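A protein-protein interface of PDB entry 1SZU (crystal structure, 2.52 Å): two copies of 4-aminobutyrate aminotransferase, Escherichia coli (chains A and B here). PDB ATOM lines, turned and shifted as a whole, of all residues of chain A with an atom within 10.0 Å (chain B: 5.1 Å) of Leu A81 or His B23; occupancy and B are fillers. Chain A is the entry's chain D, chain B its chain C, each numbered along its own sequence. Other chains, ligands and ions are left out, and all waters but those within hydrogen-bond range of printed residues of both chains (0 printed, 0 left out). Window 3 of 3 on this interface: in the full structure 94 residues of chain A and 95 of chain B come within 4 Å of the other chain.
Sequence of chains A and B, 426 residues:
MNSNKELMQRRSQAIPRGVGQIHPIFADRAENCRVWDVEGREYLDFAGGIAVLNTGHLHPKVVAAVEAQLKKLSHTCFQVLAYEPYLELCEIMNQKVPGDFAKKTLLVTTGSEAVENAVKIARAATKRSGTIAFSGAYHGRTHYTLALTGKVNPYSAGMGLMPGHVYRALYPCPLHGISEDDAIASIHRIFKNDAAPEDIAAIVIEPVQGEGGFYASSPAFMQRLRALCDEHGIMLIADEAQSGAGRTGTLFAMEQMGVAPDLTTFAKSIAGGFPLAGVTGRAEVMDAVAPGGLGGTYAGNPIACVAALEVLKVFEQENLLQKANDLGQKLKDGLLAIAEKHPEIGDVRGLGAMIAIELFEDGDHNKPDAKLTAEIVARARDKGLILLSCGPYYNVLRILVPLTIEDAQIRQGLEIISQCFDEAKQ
The side-chain amide nitrogen (NE2) of Gln B21 lies within hydrogen-bond range of the backbone carbonyl oxygen (O) of Phe A78, 2.9 Å away.
The side-chain amide nitrogen of Gln B21 lies within hydrogen-bond range of the backbone carbonyl oxygen of Val A80 (3.4 Å).
The side-chain amide nitrogen (NE2) of Gln B21 sits close to the backbone NH (N) of Ala A82 (3.4 Å).
The backbone NH (N) of Ile B22 is in hydrogen-bond range of the backbone carbonyl oxygen (O) of Gln A79 (2.7 Å).
O of Val A80 sits at hydrogen-bond distance from N of His B23.
The backbone carbonyl oxygen (O) of Ile B25 sits at hydrogen-bond distance from the backbone NH (N) of Ala A82 (2.9 Å).
The backbone NH (N) of Ala B27 is in hydrogen-bond range of the backbone carbonyl oxygen (O) of Ala A82.
The backbone carbonyl oxygen of His B23 is in hydrogen-bond range of the side-chain amide nitrogen of Gln B21 (3.1 Å).
A ring nitrogen (ND1) of His B23 is in hydrogen-bond range of the guanidinium group (NE) of Arg B381.
NE2 of His B23 is in hydrogen-bond range of O of Leu B387, 3.0 Å away.
The backbone carbonyl oxygen of Leu A81 sits at hydrogen-bond distance from the side-chain hydroxyl of Thr A76, 2.9 Å away.
The side-chain amide oxygen (OE1) of Gln A79 is in hydrogen-bond range of the backbone NH (N) of Gly A296, 2.6 Å away.
The side-chain hydroxyl (OH) of Tyr A83 lies within hydrogen-bond range of the backbone carbonyl oxygen (O) of Ala A299, at 3.3 Å.
Among the printed residues, merely in contact across the chains: Leu A73 with Ala B27 (3.9 Å), Gln A79 with Gln B21 (3.4 Å), Leu A81 with Gln B21 (3.8 Å), Leu A81 with His B23 (3.8 Å), Leu A81 with Ile B25 (3.6 Å), Leu A81 with Val B35 (3.8 Å) and Tyr A83 with Ala B27 (3.7 Å).
Of the printed residues of chain B, Leu A81 touches Gln B21, His B23, Ile B25 and Val B35.
Printed residues of chain A within 4 Å of His B23: Val A80 (3.2 Å) and Leu A81 (3.8 Å).
Gln B21 touches five residues of chain A.
Of chain A, only Gln A79 comes within 4 Å of Ile B22.
No residue of chain A comes within 4 Å of Ile B386.
Printed residues of chain A within 4 Å of Ala B27: Leu A73, Ala A82 and Tyr A83.
Printed residues of chain B within 4 Å of Tyr A83: Ala B27.
The nearest printed residue of chain B that does not touch Leu A81 is Ala B27 (4.1 Å).
The nearest residue of chain A that does not touch His B23 is Gln A79 (4.5 Å).
Of the 11 printed residues of chain B, 6 touch a printed residue of chain A.
Hydrophobic or aromatic side chains of chain B that line the printed part of chain A: Ile B22, His B23, Ile B25, Ala B27 and Val B35.
Along chain B the printed residues that touch a printed residue of chain A span positions 21 to 35.
Among the printed residues, no Asp or Glu carboxylate lies within 4 Å of a Lys or Arg side-chain nitrogen of the other chain.
No position is printed for both chains.
Of the 14 pairs that touch across the chains among the printed residues, none has its exchanged pair printed and touching as well.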
ATOM      1  N   LEU A  73     -20.084  24.772 -30.461  1.00  0.00           N
ATOM      2  CA  LEU A  73     -20.369  23.359 -30.197  1.00  0.00           C
ATOM      3  C   LEU A  73     -21.873  23.151 -30.190  1.00  0.00           C
ATOM      4  O   LEU A  73     -22.622  24.074 -29.879  1.00  0.00           O
ATOM      5  CB  LEU A  73     -19.758  22.917 -28.858  1.00  0.00           C
ATOM      6  CG  LEU A  73     -20.251  23.569 -27.562  1.00  0.00           C
ATOM      7  CD1 LEU A  73     -21.639  23.021 -27.211  1.00  0.00           C
ATOM      8  CD2 LEU A  73     -19.259  23.278 -26.428  1.00  0.00           C
ATOM      9  N   SER A  74     -22.323  21.949 -30.537  1.00  0.00           N
ATOM     10  CA  SER A  74     -23.756  21.673 -30.569  1.00  0.00           C
ATOM     11  C   SER A  74     -24.199  20.698 -29.491  1.00  0.00           C
ATOM     12  O   SER A  74     -25.390  20.602 -29.206  1.00  0.00           O
ATOM     13  CB  SER A  74     -24.173  21.120 -31.935  1.00  0.00           C
ATOM     14  OG  SER A  74     -23.731  19.774 -32.108  1.00  0.00           O
ATOM     15  N   HIS A  75     -23.253  19.983 -28.886  1.00  0.00           N
ATOM     16  CA  HIS A  75     -23.596  19.010 -27.857  1.00  0.00           C
ATOM     17  C   HIS A  75     -22.405  18.457 -27.077  1.00  0.00           C
ATOM     18  O   HIS A  75     -21.339  18.214 -27.643  1.00  0.00           O
ATOM     19  CB  HIS A  75     -24.332  17.836 -28.498  1.00  0.00           C
ATOM     20  CG  HIS A  75     -24.497  16.645 -27.594  1.00  0.00           C
ATOM     21  ND1 HIS A  75     -25.652  16.406 -26.875  1.00  0.00           N
ATOM     22  CD2 HIS A  75     -23.645  15.638 -27.286  1.00  0.00           C
ATOM     23  CE1 HIS A  75     -25.503  15.303 -26.159  1.00  0.00           C
ATOM     24  NE2 HIS A  75     -24.293  14.818 -26.389  1.00  0.00           N
ATOM     25  N   THR A  76     -22.594  18.260 -25.772  1.00  0.00           N
ATOM     26  CA  THR A  76     -21.561  17.658 -24.920  1.00  0.00           C
ATOM     27  C   THR A  76     -22.259  16.791 -23.888  1.00  0.00           C
ATOM     28  O   THR A  76     -21.631  15.899 -23.305  1.00  0.00           O
ATOM     29  CB  THR A  76     -20.761  18.678 -24.089  1.00  0.00           C
ATOM     30  OG1 THR A  76     -21.667  19.413 -23.257  1.00  0.00           O
ATOM     31  CG2 THR A  76     -19.974  19.626 -24.980  1.00  0.00           C
ATOM     32  N   CYS A  77     -23.559  17.053 -23.691  1.00  0.00           N
ATOM     33  CA  CYS A  77     -24.383  16.407 -22.660  1.00  0.00           C
ATOM     34  C   CYS A  77     -23.964  17.121 -21.350  1.00  0.00           C
ATOM     35  O   CYS A  77     -22.932  16.818 -20.747  1.00  0.00           O
ATOM     36  CB  CYS A  77     -24.120  14.900 -22.547  1.00  0.00           C
ATOM     37  SG  CYS A  77     -25.199  14.095 -21.325  1.00  0.00           S
ATOM     38  N   PHE A  78     -24.769  18.092 -20.934  1.00  0.00           N
ATOM     39  CA  PHE A  78     -24.493  18.881 -19.739  1.00  0.00           C
ATOM     40  C   PHE A  78     -23.942  18.091 -18.548  1.00  0.00           C
ATOM     41  O   PHE A  78     -22.985  18.527 -17.921  1.00  0.00           O
ATOM     42  CB  PHE A  78     -25.763  19.625 -19.326  1.00  0.00           C
ATOM     43  CG  PHE A  78     -25.528  20.731 -18.353  1.00  0.00           C
ATOM     44  CD1 PHE A  78     -25.091  21.983 -18.789  1.00  0.00           C
ATOM     45  CD2 PHE A  78     -25.768  20.538 -16.991  1.00  0.00           C
ATOM     46  CE1 PHE A  78     -24.902  23.036 -17.874  1.00  0.00           C
ATOM     47  CE2 PHE A  78     -25.583  21.575 -16.074  1.00  0.00           C
ATOM     48  CZ  PHE A  78     -25.147  22.829 -16.519  1.00  0.00           C
ATOM     49  N   GLN A  79     -24.550  16.946 -18.236  1.00  0.00           N
ATOM     50  CA  GLN A  79     -24.124  16.085 -17.120  1.00  0.00           C
ATOM     51  C   GLN A  79     -22.661  15.677 -17.161  1.00  0.00           C
ATOM     52  O   GLN A  79     -22.095  15.315 -16.127  1.00  0.00           O
ATOM     53  CB  GLN A  79     -24.932  14.798 -17.095  1.00  0.00           C
ATOM     54  CG  GLN A  79     -26.405  15.006 -17.114  1.00  0.00           C
ATOM     55  CD  GLN A  79     -27.146  13.823 -17.695  1.00  0.00           C
ATOM     56  OE1 GLN A  79     -28.217  13.997 -18.275  1.00  0.00           O
ATOM     57  NE2 GLN A  79     -26.595  12.616 -17.537  1.00  0.00           N
ATOM     58  N   VAL A  80     -22.067  15.695 -18.355  1.00  0.00           N
ATOM     59  CA  VAL A  80     -20.668  15.319 -18.537  1.00  0.00           C
ATOM     60  C   VAL A  80     -19.808  16.583 -18.487  1.00  0.00           C
ATOM     61  O   VAL A  80     -18.894  16.688 -17.658  1.00  0.00           O
ATOM     62  CB  VAL A  80     -20.466  14.571 -19.894  1.00  0.00           C
ATOM     63  CG1 VAL A  80     -19.016  14.131 -20.042  1.00  0.00           C
ATOM     64  CG2 VAL A  80     -21.403  13.360 -19.966  1.00  0.00           C
ATOM     65  N   LEU A  81     -20.095  17.529 -19.384  1.00  0.00           N
ATOM     66  CA  LEU A  81     -19.409  18.823 -19.424  1.00  0.00           C
ATOM     67  C   LEU A  81     -20.480  19.917 -19.479  1.00  0.00           C
ATOM     68  O   LEU A  81     -21.307  19.940 -20.381  1.00  0.00           O
ATOM     69  CB  LEU A  81     -18.503  18.953 -20.660  1.00  0.00           C
ATOM     70  CG  LEU A  81     -17.269  18.065 -20.803  1.00  0.00           C
ATOM     71  CD1 LEU A  81     -16.435  18.557 -21.952  1.00  0.00           C
ATOM     72  CD2 LEU A  81     -16.457  18.107 -19.550  1.00  0.00           C
ATOM     73  N   ALA A  82     -20.482  20.820 -18.516  1.00  0.00           N
ATOM     74  CA  ALA A  82     -21.466  21.893 -18.518  1.00  0.00           C
ATOM     75  C   ALA A  82     -21.112  22.891 -19.613  1.00  0.00           C
ATOM     76  O   ALA A  82     -20.098  22.752 -20.298  1.00  0.00           O
ATOM     77  CB  ALA A  82     -21.489  22.590 -17.168  1.00  0.00           C
ATOM     78  N   TYR A  83     -21.978  23.881 -19.792  1.00  0.00           N
ATOM     79  CA  TYR A  83     -21.766  24.937 -20.768  1.00  0.00           C
ATOM     80  C   TYR A  83     -22.640  26.069 -20.294  1.00  0.00           C
ATOM     81  O   TYR A  83     -23.702  25.835 -19.728  1.00  0.00           O
ATOM     82  CB  TYR A  83     -22.084  24.474 -22.223  1.00  0.00           C
ATOM     83  CG  TYR A  83     -23.263  23.536 -22.412  1.00  0.00           C
ATOM     84  CD1 TYR A  83     -24.559  24.029 -22.593  1.00  0.00           C
ATOM     85  CD2 TYR A  83     -23.082  22.152 -22.401  1.00  0.00           C
ATOM     86  CE1 TYR A  83     -25.650  23.166 -22.754  1.00  0.00           C
ATOM     87  CE2 TYR A  83     -24.161  21.278 -22.560  1.00  0.00           C
ATOM     88  CZ  TYR A  83     -25.439  21.791 -22.728  1.00  0.00           C
ATOM     89  OH  TYR A  83     -26.510  20.936 -22.804  1.00  0.00           O
ATOM     90  N   GLU A  84     -22.187  27.297 -20.504  1.00  0.00           N
ATOM     91  CA  GLU A  84     -22.896  28.477 -20.010  1.00  0.00           C
ATOM     92  C   GLU A  84     -24.340  28.720 -20.412  1.00  0.00           C
ATOM     93  O   GLU A  84     -25.163  29.091 -19.565  1.00  0.00           O
ATOM     94  CB  GLU A  84     -22.087  29.739 -20.322  1.00  0.00           C
ATOM     95  CG  GLU A  84     -20.651  29.666 -19.835  1.00  0.00           C
ATOM     96  CD  GLU A  84     -19.907  30.988 -19.959  1.00  0.00           C
ATOM     97  OE1 GLU A  84     -20.196  31.917 -19.171  1.00  0.00           O
ATOM     98  OE2 GLU A  84     -19.037  31.094 -20.844  1.00  0.00           O
ATOM     99  N   PRO A  85     -24.674  28.524 -21.702  1.00  0.00           N
ATOM    100  CA  PRO A  85     -26.045  28.751 -22.169  1.00  0.00           C
ATOM    101  C   PRO A  85     -27.085  28.043 -21.310  1.00  0.00           C
ATOM    102  O   PRO A  85     -28.106  28.622 -20.971  1.00  0.00           O
ATOM    103  CB  PRO A  85     -26.004  28.242 -23.610  1.00  0.00           C
ATOM    104  CG  PRO A  85     -24.613  28.512 -24.010  1.00  0.00           C
ATOM    105  CD  PRO A  85     -23.844  28.012 -22.803  1.00  0.00           C
ATOM    106  N   TYR A  86     -26.814  26.794 -20.959  1.00  0.00           N
ATOM    107  CA  TYR A  86     -27.730  26.030 -20.125  1.00  0.00           C
ATOM    108  C   TYR A  86     -27.845  26.747 -18.747  1.00  0.00           C
ATOM    109  O   TYR A  86     -28.936  27.112 -18.298  1.00  0.00           O
ATOM    110  CB  TYR A  86     -27.182  24.595 -20.005  1.00  0.00           C
ATOM    111  CG  TYR A  86     -28.036  23.592 -19.248  1.00  0.00           C
ATOM    112  CD1 TYR A  86     -28.373  22.366 -19.823  1.00  0.00           C
ATOM    113  CD2 TYR A  86     -28.443  23.830 -17.935  1.00  0.00           C
ATOM    114  CE1 TYR A  86     -29.088  21.403 -19.109  1.00  0.00           C
ATOM    115  CE2 TYR A  86     -29.160  22.868 -17.212  1.00  0.00           C
ATOM    116  CZ  TYR A  86     -29.482  21.661 -17.807  1.00  0.00           C
ATOM    117  OH  TYR A  86     -30.241  20.729 -17.123  1.00  0.00           O
ATOM    118  N   LEU A  87     -26.706  26.988 -18.103  1.00  0.00           N
ATOM    119  CA  LEU A  87     -26.679  27.652 -16.806  1.00  0.00           C
ATOM    120  C   LEU A  87     -27.358  28.999 -16.829  1.00  0.00           C
ATOM    121  O   LEU A  87     -28.128  29.347 -15.921  1.00  0.00           O
ATOM    122  CB  LEU A  87     -25.240  27.844 -16.339  1.00  0.00           C
ATOM    123  CG  LEU A  87     -25.053  28.756 -15.121  1.00  0.00           C
ATOM    124  CD1 LEU A  87     -25.775  28.155 -13.900  1.00  0.00           C
ATOM    125  CD2 LEU A  87     -23.559  28.934 -14.871  1.00  0.00           C
ATOM    126  N   GLY A 296     -30.605  13.187 -19.066  1.00  0.00           N
ATOM    127  CA  GLY A 296     -31.056  12.974 -20.433  1.00  0.00           C
ATOM    128  C   GLY A 296     -29.938  13.371 -21.373  1.00  0.00           C
ATOM    129  O   GLY A 296     -29.190  14.294 -21.076  1.00  0.00           O
ATOM    130  N   THR A 297     -29.834  12.703 -22.515  1.00  0.00           N
ATOM    131  CA  THR A 297     -28.760  12.989 -23.448  1.00  0.00           C
ATOM    132  C   THR A 297     -28.767  14.386 -24.071  1.00  0.00           C
ATOM    133  O   THR A 297     -27.788  15.131 -23.964  1.00  0.00           O
ATOM    134  CB  THR A 297     -28.727  11.922 -24.586  1.00  0.00           C
ATOM    135  OG1 THR A 297     -28.606  10.614 -24.011  1.00  0.00           O
ATOM    136  CG2 THR A 297     -27.535  12.153 -25.520  1.00  0.00           C
ATOM    137  N   ALA A 299     -30.789  16.881 -23.289  1.00  0.00           N
ATOM    138  CA  ALA A 299     -31.256  17.890 -22.331  1.00  0.00           C
ATOM    139  C   ALA A 299     -30.552  19.238 -22.413  1.00  0.00           C
ATOM    140  O   ALA A 299     -29.325  19.312 -22.320  1.00  0.00           O
ATOM    141  CB  ALA A 299     -31.158  17.341 -20.920  1.00  0.00           C
ATOM    142  N   GLY A 300     -31.340  20.299 -22.580  1.00  0.00           N
ATOM    143  CA  GLY A 300     -30.777  21.636 -22.662  1.00  0.00           C
ATOM    144  C   GLY A 300     -29.716  21.724 -23.738  1.00  0.00           C
ATOM    145  O   GLY A 300     -28.550  22.045 -23.484  1.00  0.00           O
ATOM    146  N   ASN A 301     -30.125  21.425 -24.957  1.00  0.00           N
ATOM    147  CA  ASN A 301     -29.226  21.468 -26.087  1.00  0.00           C
ATOM    148  C   ASN A 301     -28.659  22.881 -26.267  1.00  0.00           C
ATOM    149  O   ASN A 301     -29.412  23.876 -26.247  1.00  0.00           O
ATOM    150  CB  ASN A 301     -29.983  21.027 -27.347  1.00  0.00           C
ATOM    151  CG  ASN A 301     -29.214  21.305 -28.609  1.00  0.00           C
ATOM    152  OD1 ASN A 301     -29.357  22.372 -29.211  1.00  0.00           O
ATOM    153  ND2 ASN A 301     -28.371  20.351 -29.015  1.00  0.00           N
ATOM    154  N   PRO A 302     -27.331  22.987 -26.450  1.00  0.00           N
ATOM    155  CA  PRO A 302     -26.603  24.245 -26.642  1.00  0.00           C
ATOM    156  C   PRO A 302     -27.270  25.202 -27.622  1.00  0.00           C
ATOM    157  O   PRO A 302     -27.591  26.334 -27.257  1.00  0.00           O
ATOM    158  CB  PRO A 302     -25.242  23.779 -27.123  1.00  0.00           C
ATOM    159  CG  PRO A 302     -25.046  22.535 -26.344  1.00  0.00           C
ATOM    160  CD  PRO A 302     -26.393  21.850 -26.374  1.00  0.00           C
ATOM    161  N   GLN B  21     -22.895  16.107 -12.127  1.00  0.00           N
ATOM    162  CA  GLN B  21     -21.897  16.692 -13.005  1.00  0.00           C
ATOM    163  C   GLN B  21     -20.679  15.771 -12.962  1.00  0.00           C
ATOM    164  O   GLN B  21     -19.916  15.798 -11.996  1.00  0.00           O
ATOM    165  CB  GLN B  21     -21.516  18.081 -12.496  1.00  0.00           C
ATOM    166  CG  GLN B  21     -20.689  18.883 -13.464  1.00  0.00           C
ATOM    167  CD  GLN B  21     -21.459  19.211 -14.713  1.00  0.00           C
ATOM    168  OE1 GLN B  21     -22.488  19.891 -14.650  1.00  0.00           O
ATOM    169  NE2 GLN B  21     -20.977  18.725 -15.863  1.00  0.00           N
ATOM    170  N   ILE B  22     -20.504  14.945 -13.989  1.00  0.00           N
ATOM    171  CA  ILE B  22     -19.375  14.019 -14.025  1.00  0.00           C
ATOM    172  C   ILE B  22     -18.034  14.771 -13.930  1.00  0.00           C
ATOM    173  O   ILE B  22     -17.144  14.386 -13.164  1.00  0.00           O
ATOM    174  CB  ILE B  22     -19.397  13.178 -15.325  1.00  0.00           C
ATOM    175  CG1 ILE B  22     -20.732  12.446 -15.445  1.00  0.00           C
ATOM    176  CG2 ILE B  22     -18.242  12.175 -15.330  1.00  0.00           C
ATOM    177  CD1 ILE B  22     -20.966  11.468 -14.333  1.00  0.00           C
ATOM    178  N   HIS B  23     -17.905  15.840 -14.716  1.00  0.00           N
ATOM    179  CA  HIS B  23     -16.704  16.654 -14.743  1.00  0.00           C
ATOM    180  C   HIS B  23     -17.122  18.087 -14.452  1.00  0.00           C
ATOM    181  O   HIS B  23     -18.000  18.623 -15.120  1.00  0.00           O
ATOM    182  CB  HIS B  23     -16.058  16.555 -16.117  1.00  0.00           C
ATOM    183  CG  HIS B  23     -15.661  15.162 -16.486  1.00  0.00           C
ATOM    184  ND1 HIS B  23     -14.500  14.576 -16.034  1.00  0.00           N
ATOM    185  CD2 HIS B  23     -16.291  14.223 -17.230  1.00  0.00           C
ATOM    186  CE1 HIS B  23     -14.431  13.335 -16.482  1.00  0.00           C
ATOM    187  NE2 HIS B  23     -15.507  13.096 -17.209  1.00  0.00           N
ATOM    188  N   PRO B  24     -16.496  18.726 -13.446  1.00  0.00           N
ATOM    189  CA  PRO B  24     -16.827  20.109 -13.076  1.00  0.00           C
ATOM    190  C   PRO B  24     -16.138  21.090 -14.002  1.00  0.00           C
ATOM    191  O   PRO B  24     -15.409  21.981 -13.569  1.00  0.00           O
ATOM    192  CB  PRO B  24     -16.330  20.202 -11.638  1.00  0.00           C
ATOM    193  CG  PRO B  24     -15.073  19.393 -11.702  1.00  0.00           C
ATOM    194  CD  PRO B  24     -15.444  18.183 -12.564  1.00  0.00           C
ATOM    195  N   ILE B  25     -16.399  20.915 -15.288  1.00  0.00           N
ATOM    196  CA  ILE B  25     -15.805  21.726 -16.339  1.00  0.00           C
ATOM    197  C   ILE B  25     -16.874  22.272 -17.281  1.00  0.00           C
ATOM    198  O   ILE B  25     -17.781  21.537 -17.688  1.00  0.00           O
ATOM    199  CB  ILE B  25     -14.834  20.853 -17.158  1.00  0.00           C
ATOM    200  CG1 ILE B  25     -13.739  20.312 -16.234  1.00  0.00           C
ATOM    201  CG2 ILE B  25     -14.239  21.644 -18.299  1.00  0.00           C
ATOM    202  CD1 ILE B  25     -13.015  19.098 -16.779  1.00  0.00           C
ATOM    203  N   ALA B  27     -17.540  23.574 -20.903  1.00  0.00           N
ATOM    204  CA  ALA B  27     -17.005  23.598 -22.256  1.00  0.00           C
ATOM    205  C   ALA B  27     -17.442  24.877 -22.954  1.00  0.00           C
ATOM    206  O   ALA B  27     -18.578  25.334 -22.792  1.00  0.00           O
ATOM    207  CB  ALA B  27     -17.499  22.387 -23.038  1.00  0.00           C
ATOM    208  N   VAL B  35     -11.887  19.603 -27.182  1.00  0.00           N
ATOM    209  CA  VAL B  35     -12.807  20.449 -26.431  1.00  0.00           C
ATOM    210  C   VAL B  35     -12.018  21.461 -25.593  1.00  0.00           C
ATOM    211  O   VAL B  35     -11.050  21.102 -24.919  1.00  0.00           O
ATOM    212  CB  VAL B  35     -13.704  19.611 -25.466  1.00  0.00           C
ATOM    213  CG1 VAL B  35     -14.702  20.514 -24.776  1.00  0.00           C
ATOM    214  CG2 VAL B  35     -14.434  18.512 -26.231  1.00  0.00           C
ATOM    215  N   VAL B 377     -10.778   7.994 -13.672  1.00  0.00           N
ATOM    216  CA  VAL B 377     -11.528   9.038 -14.359  1.00  0.00           C
ATOM    217  C   VAL B 377     -11.016  10.427 -13.947  1.00  0.00           C
ATOM    218  O   VAL B 377     -10.771  11.296 -14.795  1.00  0.00           O
ATOM    219  CB  VAL B 377     -13.061   8.885 -14.077  1.00  0.00           C
ATOM    220  CG1 VAL B 377     -13.820  10.141 -14.503  1.00  0.00           C
ATOM    221  CG2 VAL B 377     -13.607   7.672 -14.839  1.00  0.00           C
ATOM    222  N   ARG B 381      -8.881  13.135 -16.160  1.00  0.00           N
ATOM    223  CA  ARG B 381      -9.359  14.516 -16.299  1.00  0.00           C
ATOM    224  C   ARG B 381      -8.204  15.487 -16.063  1.00  0.00           C
ATOM    225  O   ARG B 381      -8.045  16.458 -16.795  1.00  0.00           O
ATOM    226  CB  ARG B 381     -10.488  14.795 -15.294  1.00  0.00           C
ATOM    227  CG  ARG B 381     -11.098  16.207 -15.335  1.00  0.00           C
ATOM    228  CD  ARG B 381     -11.860  16.476 -14.034  1.00  0.00           C
ATOM    229  NE  ARG B 381     -12.766  15.377 -13.686  1.00  0.00           N
ATOM    230  CZ  ARG B 381     -13.227  15.135 -12.459  1.00  0.00           C
ATOM    231  NH1 ARG B 381     -12.867  15.913 -11.443  1.00  0.00           N
ATOM    232  NH2 ARG B 381     -14.054  14.112 -12.237  1.00  0.00           N
ATOM    233  N   ILE B 386     -11.100  13.192 -21.259  1.00  0.00           N
ATOM    234  CA  ILE B 386     -12.451  13.077 -20.708  1.00  0.00           C
ATOM    235  C   ILE B 386     -12.986  11.649 -20.871  1.00  0.00           C
ATOM    236  O   ILE B 386     -13.180  11.183 -21.991  1.00  0.00           O
ATOM    237  CB  ILE B 386     -13.406  14.048 -21.413  1.00  0.00           C
ATOM    238  CG1 ILE B 386     -12.926  15.489 -21.216  1.00  0.00           C
ATOM    239  CG2 ILE B 386     -14.825  13.847 -20.900  1.00  0.00           C
ATOM    240  CD1 ILE B 386     -12.918  15.971 -19.770  1.00  0.00           C
ATOM    241  N   LEU B 387     -13.210  10.957 -19.754  1.00  0.00           N
ATOM    242  CA  LEU B 387     -13.712   9.580 -19.787  1.00  0.00           C
ATOM    243  C   LEU B 387     -15.022   9.422 -19.015  1.00  0.00           C
ATOM    244  O   LEU B 387     -15.437  10.316 -18.272  1.00  0.00           O
ATOM    245  CB  LEU B 387     -12.699   8.605 -19.181  1.00  0.00           C
ATOM    246  CG  LEU B 387     -11.334   8.352 -19.813  1.00  0.00           C
ATOM    247  CD1 LEU B 387     -10.544   7.404 -18.927  1.00  0.00           C
ATOM    248  CD2 LEU B 387     -11.509   7.759 -21.197  1.00  0.00           C
